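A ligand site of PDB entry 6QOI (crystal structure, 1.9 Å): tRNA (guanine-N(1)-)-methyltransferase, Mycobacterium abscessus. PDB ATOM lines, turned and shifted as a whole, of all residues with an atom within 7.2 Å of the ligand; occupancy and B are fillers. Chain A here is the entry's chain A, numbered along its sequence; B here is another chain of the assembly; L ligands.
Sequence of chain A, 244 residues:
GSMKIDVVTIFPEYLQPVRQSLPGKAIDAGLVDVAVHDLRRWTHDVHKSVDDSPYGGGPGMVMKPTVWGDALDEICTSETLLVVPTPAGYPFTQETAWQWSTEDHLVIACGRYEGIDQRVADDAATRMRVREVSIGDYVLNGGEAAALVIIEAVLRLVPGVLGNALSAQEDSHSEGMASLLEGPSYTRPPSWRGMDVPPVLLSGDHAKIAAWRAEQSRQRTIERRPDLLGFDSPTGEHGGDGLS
The side-chain hydroxyl (OH) of Tyr 138 sits at hydrogen-bond distance from the backbone carbonyl oxygen (O) of Ile 135, 3.2 Å away.
The backbone NH (N) of Gly 143 lies within hydrogen-bond range of the backbone carbonyl oxygen (O) of Gly 111.
The side-chain hydroxyl of Ser 134 sits at hydrogen-bond distance from the backbone carbonyl oxygen of Gly 136, at 2.9 Å.
The backbone NH (N) of Gly 142 is in hydrogen-bond range of the side-chain carboxylate (OE2) of Glu 152 of chain B, 3.3 Å away.
N of Tyr 113 lies within hydrogen-bond range of O of Asn 141 (3.0 Å).
The backbone carbonyl oxygen (O) of Val 133 sits at hydrogen-bond distance from the backbone NH (N) of Thr 86.
N of Ala 88 lies close to OG1 of Thr 86 (3.1 Å).
A nitrogen (N2) of the ligand is in hydrogen-bond range of the backbone carbonyl oxygen (O) of Tyr 138 (2.7 Å).
The backbone NH (N) of Leu 140 lies within hydrogen-bond range of a nitrogen (N1) of the ligand (3.3 Å).
O of Gly 136 is in hydrogen-bond range of N2 of the ligand, at 3.3 Å.
Merely in contact with the ligand: Pro 85, Thr 86, Pro 87, Gly 111, Tyr 113, Ser 134, Gly 142 and Gly 143.
Hydrophobic or aromatic side chains that line the ligand: Pro 85, Pro 87, Tyr 113, Tyr 138 and Leu 140.
Within 4 Å of the ligand: Pro 85, Thr 86, Pro 87, Gly 111, Tyr 113, Ser 134, Gly 136, Tyr 138, Leu 140, Gly 142 and Gly 143.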
ATOM      1  N   VAL A  84     -13.263  24.327 -23.348  1.00  0.00           N
ATOM      2  CA  VAL A  84     -14.221  23.301 -23.725  1.00  0.00           C
ATOM      3  C   VAL A  84     -13.539  21.944 -23.599  1.00  0.00           C
ATOM      4  O   VAL A  84     -12.786  21.550 -24.481  1.00  0.00           O
ATOM      5  CB  VAL A  84     -14.761  23.470 -25.163  1.00  0.00           C
ATOM      6  CG1 VAL A  84     -15.809  22.383 -25.476  1.00  0.00           C
ATOM      7  CG2 VAL A  84     -15.364  24.874 -25.384  1.00  0.00           C
ATOM      8  N   PRO A  85     -13.752  21.261 -22.463  1.00  0.00           N
ATOM      9  CA  PRO A  85     -13.171  19.927 -22.316  1.00  0.00           C
ATOM     10  C   PRO A  85     -13.794  18.962 -23.325  1.00  0.00           C
ATOM     11  O   PRO A  85     -15.020  18.899 -23.489  1.00  0.00           O
ATOM     12  CB  PRO A  85     -13.500  19.535 -20.862  1.00  0.00           C
ATOM     13  CG  PRO A  85     -13.800  20.883 -20.160  1.00  0.00           C
ATOM     14  CD  PRO A  85     -14.409  21.730 -21.220  1.00  0.00           C
ATOM     15  N   THR A  86     -12.945  18.212 -24.020  1.00  0.00           N
ATOM     16  CA  THR A  86     -13.420  17.260 -25.016  1.00  0.00           C
ATOM     17  C   THR A  86     -12.348  16.193 -25.217  1.00  0.00           C
ATOM     18  O   THR A  86     -11.151  16.485 -25.151  1.00  0.00           O
ATOM     19  CB  THR A  86     -13.742  17.941 -26.360  1.00  0.00           C
ATOM     20  OG1 THR A  86     -13.818  16.936 -27.385  1.00  0.00           O
ATOM     21  CG2 THR A  86     -12.678  18.937 -26.718  1.00  0.00           C
ATOM     22  N   PRO A  87     -12.784  14.951 -25.426  1.00  0.00           N
ATOM     23  CA  PRO A  87     -11.797  13.896 -25.638  1.00  0.00           C
ATOM     24  C   PRO A  87     -10.996  14.105 -26.912  1.00  0.00           C
ATOM     25  O   PRO A  87      -9.943  13.503 -27.078  1.00  0.00           O
ATOM     26  CB  PRO A  87     -12.651  12.616 -25.706  1.00  0.00           C
ATOM     27  CG  PRO A  87     -14.015  13.105 -26.119  1.00  0.00           C
ATOM     28  CD  PRO A  87     -14.171  14.452 -25.485  1.00  0.00           C
ATOM     29  N   ALA A  88     -11.503  14.961 -27.799  1.00  0.00           N
ATOM     30  CA  ALA A  88     -10.827  15.255 -29.057  1.00  0.00           C
ATOM     31  C   ALA A  88      -9.994  16.526 -28.980  1.00  0.00           C
ATOM     32  O   ALA A  88      -9.630  17.098 -30.013  1.00  0.00           O
ATOM     33  CB  ALA A  88     -11.851  15.372 -30.175  1.00  0.00           C
ATOM     34  N   GLY A  89      -9.686  16.982 -27.775  1.00  0.00           N
ATOM     35  CA  GLY A  89      -9.048  18.285 -27.596  1.00  0.00           C
ATOM     36  C   GLY A  89      -7.544  18.222 -27.622  1.00  0.00           C
ATOM     37  O   GLY A  89      -6.970  17.128 -27.611  1.00  0.00           O
ATOM     38  N   ALA A 109     -17.186  25.026 -20.470  1.00  0.00           N
ATOM     39  CA  ALA A 109     -18.413  24.460 -21.016  1.00  0.00           C
ATOM     40  C   ALA A 109     -18.376  22.939 -20.935  1.00  0.00           C
ATOM     41  O   ALA A 109     -17.629  22.290 -21.682  1.00  0.00           O
ATOM     42  CB  ALA A 109     -18.639  24.927 -22.460  1.00  0.00           C
ATOM     43  N   CYS A 110     -19.141  22.368 -20.007  1.00  0.00           N
ATOM     44  CA  CYS A 110     -19.136  20.907 -19.830  1.00  0.00           C
ATOM     45  C   CYS A 110     -20.213  20.250 -20.684  1.00  0.00           C
ATOM     46  O   CYS A 110     -21.395  20.549 -20.531  1.00  0.00           O
ATOM     47  CB  CYS A 110     -19.381  20.532 -18.363  1.00  0.00           C
ATOM     48  SG  CYS A 110     -18.242  21.245 -17.181  1.00  0.00           S
ATOM     49  N   GLY A 111     -19.794  19.360 -21.581  1.00  0.00           N
ATOM     50  CA  GLY A 111     -20.740  18.619 -22.401  1.00  0.00           C
ATOM     51  C   GLY A 111     -20.505  17.124 -22.355  1.00  0.00           C
ATOM     52  O   GLY A 111     -19.492  16.672 -21.813  1.00  0.00           O
ATOM     53  N   ARG A 112     -21.427  16.360 -22.926  1.00  0.00           N
ATOM     54  CA  ARG A 112     -21.282  14.898 -23.039  1.00  0.00           C
ATOM     55  C   ARG A 112     -20.188  14.529 -24.035  1.00  0.00           C
ATOM     56  O   ARG A 112     -19.815  15.332 -24.884  1.00  0.00           O
ATOM     57  CB  ARG A 112     -22.616  14.279 -23.450  1.00  0.00           C
ATOM     58  CG  ARG A 112     -23.153  14.827 -24.760  1.00  0.00           C
ATOM     59  CD  ARG A 112     -24.613  14.436 -24.950  1.00  0.00           C
ATOM     60  NE  ARG A 112     -24.757  12.996 -25.185  1.00  0.00           N
ATOM     61  CZ  ARG A 112     -25.685  12.232 -24.611  1.00  0.00           C
ATOM     62  NH1 ARG A 112     -26.557  12.752 -23.757  1.00  0.00           N
ATOM     63  NH2 ARG A 112     -25.728  10.935 -24.890  1.00  0.00           N
ATOM     64  N   TYR A 113     -19.674  13.305 -23.948  1.00  0.00           N
ATOM     65  CA  TYR A 113     -18.478  12.955 -24.729  1.00  0.00           C
ATOM     66  C   TYR A 113     -18.729  12.986 -26.237  1.00  0.00           C
ATOM     67  O   TYR A 113     -17.804  13.229 -27.014  1.00  0.00           O
ATOM     68  CB  TYR A 113     -17.929  11.592 -24.314  1.00  0.00           C
ATOM     69  CG  TYR A 113     -18.790  10.419 -24.673  1.00  0.00           C
ATOM     70  CD1 TYR A 113     -19.916  10.092 -23.918  1.00  0.00           C
ATOM     71  CD2 TYR A 113     -18.483   9.614 -25.764  1.00  0.00           C
ATOM     72  CE1 TYR A 113     -20.709   9.004 -24.258  1.00  0.00           C
ATOM     73  CE2 TYR A 113     -19.270   8.534 -26.103  1.00  0.00           C
ATOM     74  CZ  TYR A 113     -20.382   8.222 -25.346  1.00  0.00           C
ATOM     75  OH  TYR A 113     -21.162   7.149 -25.684  1.00  0.00           O
ATOM     76  N   GLU A 114     -19.979  12.770 -26.658  1.00  0.00           N
ATOM     77  CA  GLU A 114     -20.330  12.802 -28.077  1.00  0.00           C
ATOM     78  C   GLU A 114     -20.212  14.193 -28.641  1.00  0.00           C
ATOM     79  O   GLU A 114     -20.077  14.368 -29.858  1.00  0.00           O
ATOM     80  CB  GLU A 114     -21.742  12.278 -28.329  1.00  0.00           C
ATOM     81  CG  GLU A 114     -21.994  10.891 -27.777  1.00  0.00           C
ATOM     82  CD  GLU A 114     -22.720  10.923 -26.457  1.00  0.00           C
ATOM     83  OE1 GLU A 114     -22.372  11.763 -25.606  1.00  0.00           O
ATOM     84  OE2 GLU A 114     -23.661  10.119 -26.279  1.00  0.00           O
ATOM     85  N   GLY A 115     -20.296  15.183 -27.760  1.00  0.00           N
ATOM     86  CA  GLY A 115     -19.876  16.528 -28.093  1.00  0.00           C
ATOM     87  C   GLY A 115     -20.965  17.581 -28.125  1.00  0.00           C
ATOM     88  O   GLY A 115     -22.164  17.277 -28.071  1.00  0.00           O
ATOM     89  N   VAL A 133      -9.814  21.100 -25.017  1.00  0.00           N
ATOM     90  CA  VAL A 133      -8.721  20.370 -24.370  1.00  0.00           C
ATOM     91  C   VAL A 133      -9.168  19.062 -23.762  1.00  0.00           C
ATOM     92  O   VAL A 133     -10.290  18.925 -23.279  1.00  0.00           O
ATOM     93  CB  VAL A 133      -8.039  21.212 -23.242  1.00  0.00           C
ATOM     94  CG1 VAL A 133      -7.269  22.410 -23.826  1.00  0.00           C
ATOM     95  CG2 VAL A 133      -9.080  21.662 -22.187  1.00  0.00           C
ATOM     96  N   SER A 134      -8.259  18.086 -23.796  1.00  0.00           N
ATOM     97  CA  SER A 134      -8.474  16.791 -23.163  1.00  0.00           C
ATOM     98  C   SER A 134      -7.541  16.656 -21.978  1.00  0.00           C
ATOM     99  O   SER A 134      -6.356  16.994 -22.099  1.00  0.00           O
ATOM    100  CB  SER A 134      -8.198  15.648 -24.147  1.00  0.00           C
ATOM    101  OG  SER A 134      -8.184  14.420 -23.445  1.00  0.00           O
ATOM    102  N   ILE A 135      -8.045  16.174 -20.837  1.00  0.00           N
ATOM    103  CA  ILE A 135      -7.188  15.989 -19.677  1.00  0.00           C
ATOM    104  C   ILE A 135      -6.449  14.645 -19.659  1.00  0.00           C
ATOM    105  O   ILE A 135      -5.683  14.379 -18.730  1.00  0.00           O
ATOM    106  CB  ILE A 135      -7.945  16.105 -18.360  1.00  0.00           C
ATOM    107  CG1 ILE A 135      -9.095  15.084 -18.296  1.00  0.00           C
ATOM    108  CG2 ILE A 135      -8.438  17.550 -18.143  1.00  0.00           C
ATOM    109  CD1 ILE A 135      -9.612  14.805 -16.904  1.00  0.00           C
ATOM    110  N   GLY A 136      -6.680  13.796 -20.661  1.00  0.00           N
ATOM    111  CA  GLY A 136      -6.012  12.497 -20.700  1.00  0.00           C
ATOM    112  C   GLY A 136      -6.522  11.559 -21.785  1.00  0.00           C
ATOM    113  O   GLY A 136      -7.547  11.828 -22.416  1.00  0.00           O
ATOM    114  N   ASP A 137      -5.809  10.458 -22.005  1.00  0.00           N
ATOM    115  CA  ASP A 137      -6.163   9.524 -23.067  1.00  0.00           C
ATOM    116  C   ASP A 137      -7.085   8.447 -22.554  1.00  0.00           C
ATOM    117  O   ASP A 137      -6.748   7.257 -22.536  1.00  0.00           O
ATOM    118  CB  ASP A 137      -4.916   8.876 -23.687  1.00  0.00           C
ATOM    119  CG  ASP A 137      -4.138   9.827 -24.566  1.00  0.00           C
ATOM    120  OD1 ASP A 137      -4.767  10.651 -25.257  1.00  0.00           O
ATOM    121  OD2 ASP A 137      -2.897   9.742 -24.557  1.00  0.00           O
ATOM    122  N   TYR A 138      -8.250   8.875 -22.116  1.00  0.00           N
ATOM    123  CA  TYR A 138      -9.291   7.971 -21.677  1.00  0.00           C
ATOM    124  C   TYR A 138     -10.588   8.686 -21.976  1.00  0.00           C
ATOM    125  O   TYR A 138     -10.595   9.901 -22.258  1.00  0.00           O
ATOM    126  CB  TYR A 138      -9.176   7.630 -20.192  1.00  0.00           C
ATOM    127  CG  TYR A 138      -8.700   8.822 -19.383  1.00  0.00           C
ATOM    128  CD1 TYR A 138      -9.569   9.862 -19.041  1.00  0.00           C
ATOM    129  CD2 TYR A 138      -7.374   8.915 -18.974  1.00  0.00           C
ATOM    130  CE1 TYR A 138      -9.109  10.982 -18.311  1.00  0.00           C
ATOM    131  CE2 TYR A 138      -6.914  10.034 -18.233  1.00  0.00           C
ATOM    132  CZ  TYR A 138      -7.789  11.055 -17.923  1.00  0.00           C
ATOM    133  OH  TYR A 138      -7.321  12.142 -17.206  1.00  0.00           O
ATOM    134  N   VAL A 139     -11.685   7.959 -21.913  1.00  0.00           N
ATOM    135  CA  VAL A 139     -12.977   8.547 -22.214  1.00  0.00           C
ATOM    136  C   VAL A 139     -13.859   8.637 -20.972  1.00  0.00           C
ATOM    137  O   VAL A 139     -14.031   7.649 -20.258  1.00  0.00           O
ATOM    138  CB  VAL A 139     -13.733   7.741 -23.300  1.00  0.00           C
ATOM    139  CG1 VAL A 139     -15.104   8.343 -23.561  1.00  0.00           C
ATOM    140  CG2 VAL A 139     -12.901   7.688 -24.580  1.00  0.00           C
ATOM    141  N   LEU A 140     -14.357   9.836 -20.719  1.00  0.00           N
ATOM    142  CA  LEU A 140     -15.335  10.091 -19.673  1.00  0.00           C
ATOM    143  C   LEU A 140     -16.679  10.208 -20.343  1.00  0.00           C
ATOM    144  O   LEU A 140     -16.745  10.444 -21.547  1.00  0.00           O
ATOM    145  CB  LEU A 140     -15.017  11.395 -18.926  1.00  0.00           C
ATOM    146  CG  LEU A 140     -13.578  11.454 -18.407  1.00  0.00           C
ATOM    147  CD1 LEU A 140     -13.317  12.742 -17.663  1.00  0.00           C
ATOM    148  CD2 LEU A 140     -13.292  10.254 -17.517  1.00  0.00           C
ATOM    149  N   ASN A 141     -17.750  10.087 -19.566  1.00  0.00           N
ATOM    150  CA  ASN A 141     -19.078  10.286 -20.128  1.00  0.00           C
ATOM    151  C   ASN A 141     -19.401  11.761 -20.358  1.00  0.00           C
ATOM    152  O   ASN A 141     -20.192  12.099 -21.240  1.00  0.00           O
ATOM    153  CB  ASN A 141     -20.125   9.676 -19.208  1.00  0.00           C
ATOM    154  CG  ASN A 141     -21.022   8.717 -19.959  1.00  0.00           C
ATOM    155  OD1 ASN A 141     -20.536   7.824 -20.654  1.00  0.00           O
ATOM    156  ND2 ASN A 141     -22.335   8.922 -19.846  1.00  0.00           N
ATOM    157  N   GLY A 142     -18.792  12.641 -19.579  1.00  0.00           N
ATOM    158  CA  GLY A 142     -19.095  14.065 -19.653  1.00  0.00           C
ATOM    159  C   GLY A 142     -17.912  14.902 -19.212  1.00  0.00           C
ATOM    160  O   GLY A 142     -16.961  14.393 -18.626  1.00  0.00           O
ATOM    161  N   GLY A 143     -17.965  16.199 -19.476  1.00  0.00           N
ATOM    162  CA  GLY A 143     -16.860  17.109 -19.149  1.00  0.00           C
ATOM    163  C   GLY A 143     -16.704  17.513 -17.700  1.00  0.00           C
ATOM    164  O   GLY A 143     -15.709  18.138 -17.353  1.00  0.00           O
ATOM    165  N   GLU A 144     -17.676  17.168 -16.844  1.00  0.00           N
ATOM    166  CA  GLU A 144     -17.677  17.643 -15.460  1.00  0.00           C
ATOM    167  C   GLU A 144     -16.402  17.264 -14.686  1.00  0.00           C
ATOM    168  O   GLU A 144     -15.768  18.125 -14.069  1.00  0.00           O
ATOM    169  CB  GLU A 144     -18.915  17.107 -14.726  1.00  0.00           C
ATOM    170  CG  GLU A 144     -20.220  17.861 -15.062  1.00  0.00           C
ATOM    171  CD  GLU A 144     -20.797  17.511 -16.441  1.00  0.00           C
ATOM    172  OE1 GLU A 144     -20.440  16.450 -17.004  1.00  0.00           O
ATOM    173  OE2 GLU A 144     -21.605  18.318 -16.956  1.00  0.00           O
ATOM    174  N   ALA A 146     -13.548  16.534 -15.894  1.00  0.00           N
ATOM    175  CA  ALA A 146     -12.433  17.253 -16.520  1.00  0.00           C
ATOM    176  C   ALA A 146     -12.379  18.708 -16.034  1.00  0.00           C
ATOM    177  O   ALA A 146     -11.294  19.280 -15.831  1.00  0.00           O
ATOM    178  CB  ALA A 146     -12.545  17.185 -18.046  1.00  0.00           C
ATOM    179  N   ALA A 147     -13.553  19.295 -15.841  1.00  0.00           N
ATOM    180  CA  ALA A 147     -13.680  20.652 -15.307  1.00  0.00           C
ATOM    181  C   ALA A 147     -13.086  20.751 -13.902  1.00  0.00           C
ATOM    182  O   ALA A 147     -12.343  21.682 -13.578  1.00  0.00           O
ATOM    183  CB  ALA A 147     -15.155  21.087 -15.294  1.00  0.00           C
ATOM    184  N   VAL B 149     -12.102  10.974 -11.691  1.00  0.00           N
ATOM    185  CA  VAL B 149     -11.825  10.711 -13.090  1.00  0.00           C
ATOM    186  C   VAL B 149     -11.726   9.210 -13.327  1.00  0.00           C
ATOM    187  O   VAL B 149     -12.353   8.648 -14.246  1.00  0.00           O
ATOM    188  CB  VAL B 149     -10.534  11.385 -13.547  1.00  0.00           C
ATOM    189  CG1 VAL B 149     -10.055  10.773 -14.858  1.00  0.00           C
ATOM    190  CG2 VAL B 149     -10.755  12.904 -13.681  1.00  0.00           C
ATOM    191  N   GLU B 152     -15.121   7.412 -13.041  1.00  0.00           N
ATOM    192  CA  GLU B 152     -16.016   7.629 -14.167  1.00  0.00           C
ATOM    193  C   GLU B 152     -15.560   6.867 -15.412  1.00  0.00           C
ATOM    194  O   GLU B 152     -16.381   6.316 -16.152  1.00  0.00           O
ATOM    195  CB  GLU B 152     -16.133   9.127 -14.483  1.00  0.00           C
ATOM    196  CG  GLU B 152     -16.999   9.396 -15.705  1.00  0.00           C
ATOM    197  CD  GLU B 152     -17.676  10.743 -15.651  1.00  0.00           C
ATOM    198  OE1 GLU B 152     -17.602  11.417 -14.598  1.00  0.00           O
ATOM    199  OE2 GLU B 152     -18.282  11.131 -16.676  1.00  0.00           O
HETATM  200  C1  LIG L   1     -14.770  15.974 -21.916  1.00  0.00           C
HETATM  201  N1  LIG L   1     -13.180  12.659 -21.961  1.00  0.00           N
HETATM  202  S1  LIG L   1     -12.107  14.927 -21.650  1.00  0.00           S
HETATM  203  C2  LIG L   1     -16.120  15.661 -22.117  1.00  0.00           C
HETATM  204  N2  LIG L   1     -10.718  12.546 -21.656  1.00  0.00           N
HETATM  205  C3  LIG L   1     -16.510  14.329 -22.264  1.00  0.00           C
HETATM  206  C4  LIG L   1     -15.572  13.318 -22.220  1.00  0.00           C
HETATM  207  C5  LIG L   1     -14.194  13.619 -22.020  1.00  0.00           C
HETATM  208  C6  LIG L   1     -13.824  14.942 -21.874  1.00  0.00           C
HETATM  209  C7  LIG L   1     -11.959  13.203 -21.769  1.00  0.00           C
